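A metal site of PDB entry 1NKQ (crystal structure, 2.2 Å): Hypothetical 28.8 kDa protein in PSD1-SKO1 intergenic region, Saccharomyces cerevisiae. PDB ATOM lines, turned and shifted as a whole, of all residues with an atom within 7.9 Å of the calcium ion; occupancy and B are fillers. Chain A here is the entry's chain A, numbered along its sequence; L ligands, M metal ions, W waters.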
ATOM      1  N   CYS A  14       8.130  17.705  10.784  1.00  0.00           N
ATOM      2  CA  CYS A  14       7.272  16.952   9.876  1.00  0.00           C
ATOM      3  C   CYS A  14       6.827  15.620  10.472  1.00  0.00           C
ATOM      4  O   CYS A  14       7.547  15.018  11.269  1.00  0.00           O
ATOM      5  CB  CYS A  14       8.021  16.704   8.570  1.00  0.00           C
ATOM      6  SG  CYS A  14       9.031  18.120   8.018  1.00  0.00           S
ATOM      7  N   ILE A  15       5.631  15.176  10.082  1.00  0.00           N
ATOM      8  CA  ILE A  15       5.088  13.904  10.544  1.00  0.00           C
ATOM      9  C   ILE A  15       5.127  12.979   9.329  1.00  0.00           C
ATOM     10  O   ILE A  15       4.877  13.432   8.206  1.00  0.00           O
ATOM     11  CB  ILE A  15       3.620  14.066  11.037  1.00  0.00           C
ATOM     12  CG1 ILE A  15       3.178  12.790  11.773  1.00  0.00           C
ATOM     13  CG2 ILE A  15       2.678  14.325   9.849  1.00  0.00           C
ATOM     14  CD1 ILE A  15       1.848  12.900  12.454  1.00  0.00           C
ATOM     15  N   GLY A  16       5.438  11.703   9.526  1.00  0.00           N
ATOM     16  CA  GLY A  16       5.501  10.786   8.407  1.00  0.00           C
ATOM     17  C   GLY A  16       4.280   9.900   8.280  1.00  0.00           C
ATOM     18  O   GLY A  16       3.388   9.982   9.100  1.00  0.00           O
ATOM     19  N   ARG A  17       4.251   9.050   7.247  1.00  0.00           N
ATOM     20  CA  ARG A  17       3.143   8.126   6.982  1.00  0.00           C
ATOM     21  C   ARG A  17       1.878   8.593   7.722  1.00  0.00           C
ATOM     22  O   ARG A  17       1.489   7.982   8.729  1.00  0.00           O
ATOM     23  CB  ARG A  17       3.529   6.721   7.469  1.00  0.00           C
ATOM     24  CG  ARG A  17       4.826   6.199   6.832  1.00  0.00           C
ATOM     25  CD  ARG A  17       5.354   4.973   7.571  1.00  0.00           C
ATOM     26  NE  ARG A  17       6.740   4.698   7.204  1.00  0.00           N
ATOM     27  CZ  ARG A  17       7.653   4.205   8.030  1.00  0.00           C
ATOM     28  NH1 ARG A  17       7.329   3.936   9.292  1.00  0.00           N
ATOM     29  NH2 ARG A  17       8.909   4.010   7.618  1.00  0.00           N
ATOM     30  N   ASN A  18       1.244   9.648   7.207  1.00  0.00           N
ATOM     31  CA  ASN A  18       0.052  10.227   7.824  1.00  0.00           C
ATOM     32  C   ASN A  18      -1.181  10.247   6.918  1.00  0.00           C
ATOM     33  O   ASN A  18      -2.115  11.026   7.151  1.00  0.00           O
ATOM     34  CB  ASN A  18       0.400  11.653   8.291  1.00  0.00           C
ATOM     35  CG  ASN A  18      -0.585  12.181   9.310  1.00  0.00           C
ATOM     36  OD1 ASN A  18      -0.729  13.405   9.467  1.00  0.00           O
ATOM     37  ND2 ASN A  18      -1.235  11.284  10.033  1.00  0.00           N
ATOM     38  N   PHE A  35       5.650   9.162  13.710  1.00  0.00           N
ATOM     39  CA  PHE A  35       7.026   9.561  13.941  1.00  0.00           C
ATOM     40  C   PHE A  35       7.261  10.939  13.337  1.00  0.00           C
ATOM     41  O   PHE A  35       6.522  11.375  12.449  1.00  0.00           O
ATOM     42  CB  PHE A  35       7.996   8.528  13.343  1.00  0.00           C
ATOM     43  CG  PHE A  35       7.920   8.378  11.854  1.00  0.00           C
ATOM     44  CD1 PHE A  35       8.660   9.207  11.009  1.00  0.00           C
ATOM     45  CD2 PHE A  35       7.132   7.387  11.280  1.00  0.00           C
ATOM     46  CE1 PHE A  35       8.614   9.045   9.628  1.00  0.00           C
ATOM     47  CE2 PHE A  35       7.079   7.211   9.904  1.00  0.00           C
ATOM     48  CZ  PHE A  35       7.823   8.043   9.073  1.00  0.00           C
ATOM     49  N   PHE A  37      10.325  14.161  12.166  1.00  0.00           N
ATOM     50  CA  PHE A  37      11.684  14.507  11.756  1.00  0.00           C
ATOM     51  C   PHE A  37      11.777  16.004  11.433  1.00  0.00           C
ATOM     52  O   PHE A  37      10.766  16.640  11.129  1.00  0.00           O
ATOM     53  CB  PHE A  37      12.103  13.665  10.549  1.00  0.00           C
ATOM     54  CG  PHE A  37      11.176  13.767   9.363  1.00  0.00           C
ATOM     55  CD1 PHE A  37      11.322  14.792   8.431  1.00  0.00           C
ATOM     56  CD2 PHE A  37      10.168  12.836   9.165  1.00  0.00           C
ATOM     57  CE1 PHE A  37      10.467  14.883   7.322  1.00  0.00           C
ATOM     58  CE2 PHE A  37       9.308  12.921   8.068  1.00  0.00           C
ATOM     59  CZ  PHE A  37       9.457  13.949   7.149  1.00  0.00           C
ATOM     60  N   LYS A  39      13.573  19.477   9.374  1.00  0.00           N
ATOM     61  CA  LYS A  39      14.098  19.911   8.086  1.00  0.00           C
ATOM     62  C   LYS A  39      14.750  21.257   8.344  1.00  0.00           C
ATOM     63  O   LYS A  39      14.221  22.086   9.077  1.00  0.00           O
ATOM     64  CB  LYS A  39      12.985  20.077   7.049  1.00  0.00           C
ATOM     65  CG  LYS A  39      12.774  18.861   6.191  1.00  0.00           C
ATOM     66  CD  LYS A  39      12.093  19.212   4.889  1.00  0.00           C
ATOM     67  CE  LYS A  39      12.255  18.097   3.877  1.00  0.00           C
ATOM     68  NZ  LYS A  39      11.436  18.328   2.668  1.00  0.00           N
ATOM     69  N   HIS A  86       9.316  13.080  -4.583  1.00  0.00           N
ATOM     70  CA  HIS A  86       8.502  14.228  -4.228  1.00  0.00           C
ATOM     71  C   HIS A  86       7.355  13.807  -3.320  1.00  0.00           C
ATOM     72  O   HIS A  86       6.811  12.704  -3.459  1.00  0.00           O
ATOM     73  CB  HIS A  86       7.956  14.914  -5.490  1.00  0.00           C
ATOM     74  CG  HIS A  86       7.153  14.008  -6.372  1.00  0.00           C
ATOM     75  ND1 HIS A  86       5.884  13.600  -6.054  1.00  0.00           N
ATOM     76  CD2 HIS A  86       7.458  13.410  -7.545  1.00  0.00           C
ATOM     77  CE1 HIS A  86       5.435  12.789  -6.998  1.00  0.00           C
ATOM     78  NE2 HIS A  86       6.372  12.652  -7.912  1.00  0.00           N
ATOM     79  N   GLU A  87       6.993  14.678  -2.386  1.00  0.00           N
ATOM     80  CA  GLU A  87       5.896  14.431  -1.445  1.00  0.00           C
ATOM     81  C   GLU A  87       5.149  15.733  -1.221  1.00  0.00           C
ATOM     82  O   GLU A  87       5.606  16.595  -0.476  1.00  0.00           O
ATOM     83  CB  GLU A  87       6.447  13.938  -0.094  1.00  0.00           C
ATOM     84  CG  GLU A  87       7.301  12.689  -0.161  1.00  0.00           C
ATOM     85  CD  GLU A  87       7.511  12.061   1.219  1.00  0.00           C
ATOM     86  OE1 GLU A  87       7.799  12.813   2.179  1.00  0.00           O
ATOM     87  OE2 GLU A  87       7.402  10.826   1.329  1.00  0.00           O
ATOM     88  N   ILE A  88       3.989  15.879  -1.868  1.00  0.00           N
ATOM     89  CA  ILE A  88       3.218  17.101  -1.700  1.00  0.00           C
ATOM     90  C   ILE A  88       2.525  17.070  -0.338  1.00  0.00           C
ATOM     91  O   ILE A  88       1.937  16.051   0.032  1.00  0.00           O
ATOM     92  CB  ILE A  88       2.182  17.296  -2.840  1.00  0.00           C
ATOM     93  CG1 ILE A  88       1.487  18.648  -2.669  1.00  0.00           C
ATOM     94  CG2 ILE A  88       1.193  16.138  -2.866  1.00  0.00           C
ATOM     95  CD1 ILE A  88       2.412  19.830  -2.958  1.00  0.00           C
ATOM     96  N   GLU A  89       2.617  18.165   0.399  1.00  0.00           N
ATOM     97  CA  GLU A  89       2.045  18.228   1.735  1.00  0.00           C
ATOM     98  C   GLU A  89       1.508  19.588   2.164  1.00  0.00           C
ATOM     99  O   GLU A  89       1.910  20.621   1.641  1.00  0.00           O
ATOM    100  CB  GLU A  89       3.110  17.796   2.754  1.00  0.00           C
ATOM    101  CG  GLU A  89       3.655  16.398   2.539  1.00  0.00           C
ATOM    102  CD  GLU A  89       4.693  16.002   3.582  1.00  0.00           C
ATOM    103  OE1 GLU A  89       4.541  16.419   4.747  1.00  0.00           O
ATOM    104  OE2 GLU A  89       5.642  15.260   3.227  1.00  0.00           O
ATOM    105  N   LEU A 120       6.629  20.935  -0.597  1.00  0.00           N
ATOM    106  CA  LEU A 120       7.101  19.661  -1.095  1.00  0.00           C
ATOM    107  C   LEU A 120       8.156  19.153  -0.122  1.00  0.00           C
ATOM    108  O   LEU A 120       9.102  19.851   0.200  1.00  0.00           O
ATOM    109  CB  LEU A 120       7.744  19.797  -2.481  1.00  0.00           C
ATOM    110  CG  LEU A 120       6.871  19.819  -3.743  1.00  0.00           C
ATOM    111  CD1 LEU A 120       7.721  20.243  -4.933  1.00  0.00           C
ATOM    112  CD2 LEU A 120       6.279  18.456  -3.986  1.00  0.00           C
ATOM    113  N   ASP A 121       7.965  17.932   0.351  1.00  0.00           N
ATOM    114  CA  ASP A 121       8.927  17.306   1.246  1.00  0.00           C
ATOM    115  C   ASP A 121       9.781  16.380   0.386  1.00  0.00           C
ATOM    116  O   ASP A 121       9.484  15.188   0.259  1.00  0.00           O
ATOM    117  CB  ASP A 121       8.194  16.523   2.323  1.00  0.00           C
ATOM    118  CG  ASP A 121       9.139  15.743   3.224  1.00  0.00           C
ATOM    119  OD1 ASP A 121      10.303  16.176   3.351  1.00  0.00           O
ATOM    120  OD2 ASP A 121       8.711  14.729   3.798  1.00  0.00           O
ATOM    121  N   LEU A 122      10.840  16.928  -0.209  1.00  0.00           N
ATOM    122  CA  LEU A 122      11.724  16.161  -1.065  1.00  0.00           C
ATOM    123  C   LEU A 122      12.679  15.287  -0.245  1.00  0.00           C
ATOM    124  O   LEU A 122      13.229  15.712   0.766  1.00  0.00           O
ATOM    125  CB  LEU A 122      12.517  17.097  -2.001  1.00  0.00           C
ATOM    126  CG  LEU A 122      11.621  17.982  -2.890  1.00  0.00           C
ATOM    127  CD1 LEU A 122      12.461  18.741  -3.913  1.00  0.00           C
ATOM    128  CD2 LEU A 122      10.591  17.117  -3.596  1.00  0.00           C
ATOM    129  N   THR A 123      12.872  14.056  -0.709  1.00  0.00           N
ATOM    130  CA  THR A 123      13.718  13.101   0.000  1.00  0.00           C
ATOM    131  C   THR A 123      14.718  12.368  -0.883  1.00  0.00           C
ATOM    132  O   THR A 123      14.398  11.985  -2.015  1.00  0.00           O
ATOM    133  CB  THR A 123      12.859  12.035   0.697  1.00  0.00           C
ATOM    134  OG1 THR A 123      11.764  12.665   1.384  1.00  0.00           O
ATOM    135  CG2 THR A 123      13.698  11.241   1.684  1.00  0.00           C
ATOM    136  N   TRP A 138      18.036  10.637   9.455  1.00  0.00           N
ATOM    137  CA  TRP A 138      17.461  10.975   8.150  1.00  0.00           C
ATOM    138  C   TRP A 138      17.811  12.405   7.723  1.00  0.00           C
ATOM    139  O   TRP A 138      17.511  12.798   6.594  1.00  0.00           O
ATOM    140  CB  TRP A 138      15.937  10.906   8.204  1.00  0.00           C
ATOM    141  CG  TRP A 138      15.321   9.569   8.423  1.00  0.00           C
ATOM    142  CD1 TRP A 138      15.908   8.449   8.940  1.00  0.00           C
ATOM    143  CD2 TRP A 138      13.964   9.223   8.142  1.00  0.00           C
ATOM    144  NE1 TRP A 138      15.000   7.421   8.992  1.00  0.00           N
ATOM    145  CE2 TRP A 138      13.797   7.867   8.502  1.00  0.00           C
ATOM    146  CE3 TRP A 138      12.864   9.925   7.614  1.00  0.00           C
ATOM    147  CZ2 TRP A 138      12.572   7.195   8.354  1.00  0.00           C
ATOM    148  CZ3 TRP A 138      11.648   9.254   7.463  1.00  0.00           C
ATOM    149  CH2 TRP A 138      11.518   7.907   7.839  1.00  0.00           C
ATOM    150  N   LYS A 142      16.825  14.359   4.114  1.00  0.00           N
ATOM    151  CA  LYS A 142      15.671  15.232   4.146  1.00  0.00           C
ATOM    152  C   LYS A 142      16.068  16.706   4.177  1.00  0.00           C
ATOM    153  O   LYS A 142      15.211  17.584   4.060  1.00  0.00           O
ATOM    154  CB  LYS A 142      14.825  14.926   5.376  1.00  0.00           C
ATOM    155  CG  LYS A 142      14.093  13.596   5.341  1.00  0.00           C
ATOM    156  CD  LYS A 142      12.797  13.713   4.579  1.00  0.00           C
ATOM    157  CE  LYS A 142      11.905  12.511   4.777  1.00  0.00           C
ATOM    158  NZ  LYS A 142      10.603  12.684   4.042  1.00  0.00           N
ATOM    159  N   LEU A 213       4.854  20.324   8.690  1.00  0.00           N
ATOM    160  CA  LEU A 213       4.449  19.599   7.479  1.00  0.00           C
ATOM    161  C   LEU A 213       3.560  18.473   7.995  1.00  0.00           C
ATOM    162  O   LEU A 213       3.928  17.779   8.944  1.00  0.00           O
ATOM    163  CB  LEU A 213       5.679  19.079   6.719  1.00  0.00           C
ATOM    164  CG  LEU A 213       6.591  20.163   6.113  1.00  0.00           C
ATOM    165  CD1 LEU A 213       7.567  19.531   5.130  1.00  0.00           C
ATOM    166  CD2 LEU A 213       5.755  21.206   5.394  1.00  0.00           C
ATOM    167  N   THR A 214       2.401  18.277   7.385  1.00  0.00           N
ATOM    168  CA  THR A 214       1.458  17.288   7.901  1.00  0.00           C
ATOM    169  C   THR A 214       1.300  15.937   7.212  1.00  0.00           C
ATOM    170  O   THR A 214       0.330  15.218   7.487  1.00  0.00           O
ATOM    171  CB  THR A 214       0.070  17.930   8.057  1.00  0.00           C
ATOM    172  OG1 THR A 214      -0.419  18.320   6.763  1.00  0.00           O
ATOM    173  CG2 THR A 214       0.161  19.169   8.943  1.00  0.00           C
ATOM    174  N   GLY A 215       2.222  15.584   6.325  1.00  0.00           N
ATOM    175  CA  GLY A 215       2.133  14.301   5.664  1.00  0.00           C
ATOM    176  C   GLY A 215       1.760  14.395   4.211  1.00  0.00           C
ATOM    177  O   GLY A 215       1.220  15.405   3.766  1.00  0.00           O
ATOM    178  N   THR A 216       2.019  13.333   3.475  1.00  0.00           N
ATOM    179  CA  THR A 216       1.721  13.306   2.048  1.00  0.00           C
ATOM    180  C   THR A 216       0.828  12.117   1.667  1.00  0.00           C
ATOM    181  O   THR A 216       0.860  11.082   2.324  1.00  0.00           O
ATOM    182  CB  THR A 216       3.036  13.236   1.248  1.00  0.00           C
ATOM    183  OG1 THR A 216       2.789  13.561  -0.129  1.00  0.00           O
ATOM    184  CG2 THR A 216       3.639  11.832   1.337  1.00  0.00           C
HETATM  185  C1  LIG L   1       6.067  11.240   4.826  1.00  0.00           C
HETATM  186  O1  LIG L   1       7.340  11.037   5.041  1.00  0.00           O
HETATM  187  O2  LIG L   1       5.438  12.352   4.833  1.00  0.00           O
HETATM  188  C2  LIG L   1       5.288   9.969   4.532  1.00  0.00           C
HETATM  189 CA    CA M   1       6.860  13.912   4.472  1.00  0.00          CA
HETATM  190  O   HOH W   1       6.024  14.961   6.456  1.00  0.00           O
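The calcium ion is bound by the side-chain carboxylate (OD2) of Asp 121 (2.1 Å), an oxygen (O2) of the ligand (2.1 Å), the side-chain carboxylate (OE2) of Glu 89 (2.2 Å), water W1 (2.4 Å) and the side-chain carboxylate (OE1) of Glu 87 (2.7 Å). Slightly farther from the calcium ion lies O1 of the ligand (3.0 Å).
The side-chain carboxylate (OD1) of Asp 121 is in salt-bridge range of the side-chain amino group (NZ) of Lys 142 (3.6 Å). The side-chain carboxylate (OD1) of Asp 121 lies within salt-bridge range of the side-chain amino group (NZ) of Lys 39 (2.5 Å). The side-chain carboxylate (OE1) of Glu 89 sits at hydrogen-bond distance from the backbone NH (N) of Gly 215. The side-chain amino group of Lys 142 sits close to the side-chain carboxylate of Glu 87 (3.4 Å). The backbone carbonyl oxygen of Phe 37 lies within hydrogen-bond range of the backbone NH of Cys 14, at 2.9 Å. The side-chain hydroxyl (OG1) of Thr 123 is in hydrogen-bond range of the side-chain amino group (NZ) of Lys 142 (2.9 Å).
Merely in contact with the calcium ion: Phe 37 (3.7 Å) and Lys 142 (3.96 Å). Five residues have an atom within 4 Å of the calcium ion: Phe 37, Glu 87, Glu 89, Asp 121 and Lys 142.
Water W1 lies within hydrogen-bond range of O of Ile 15 (2.6 Å) and OE1 of Glu 89 (2.7 Å).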
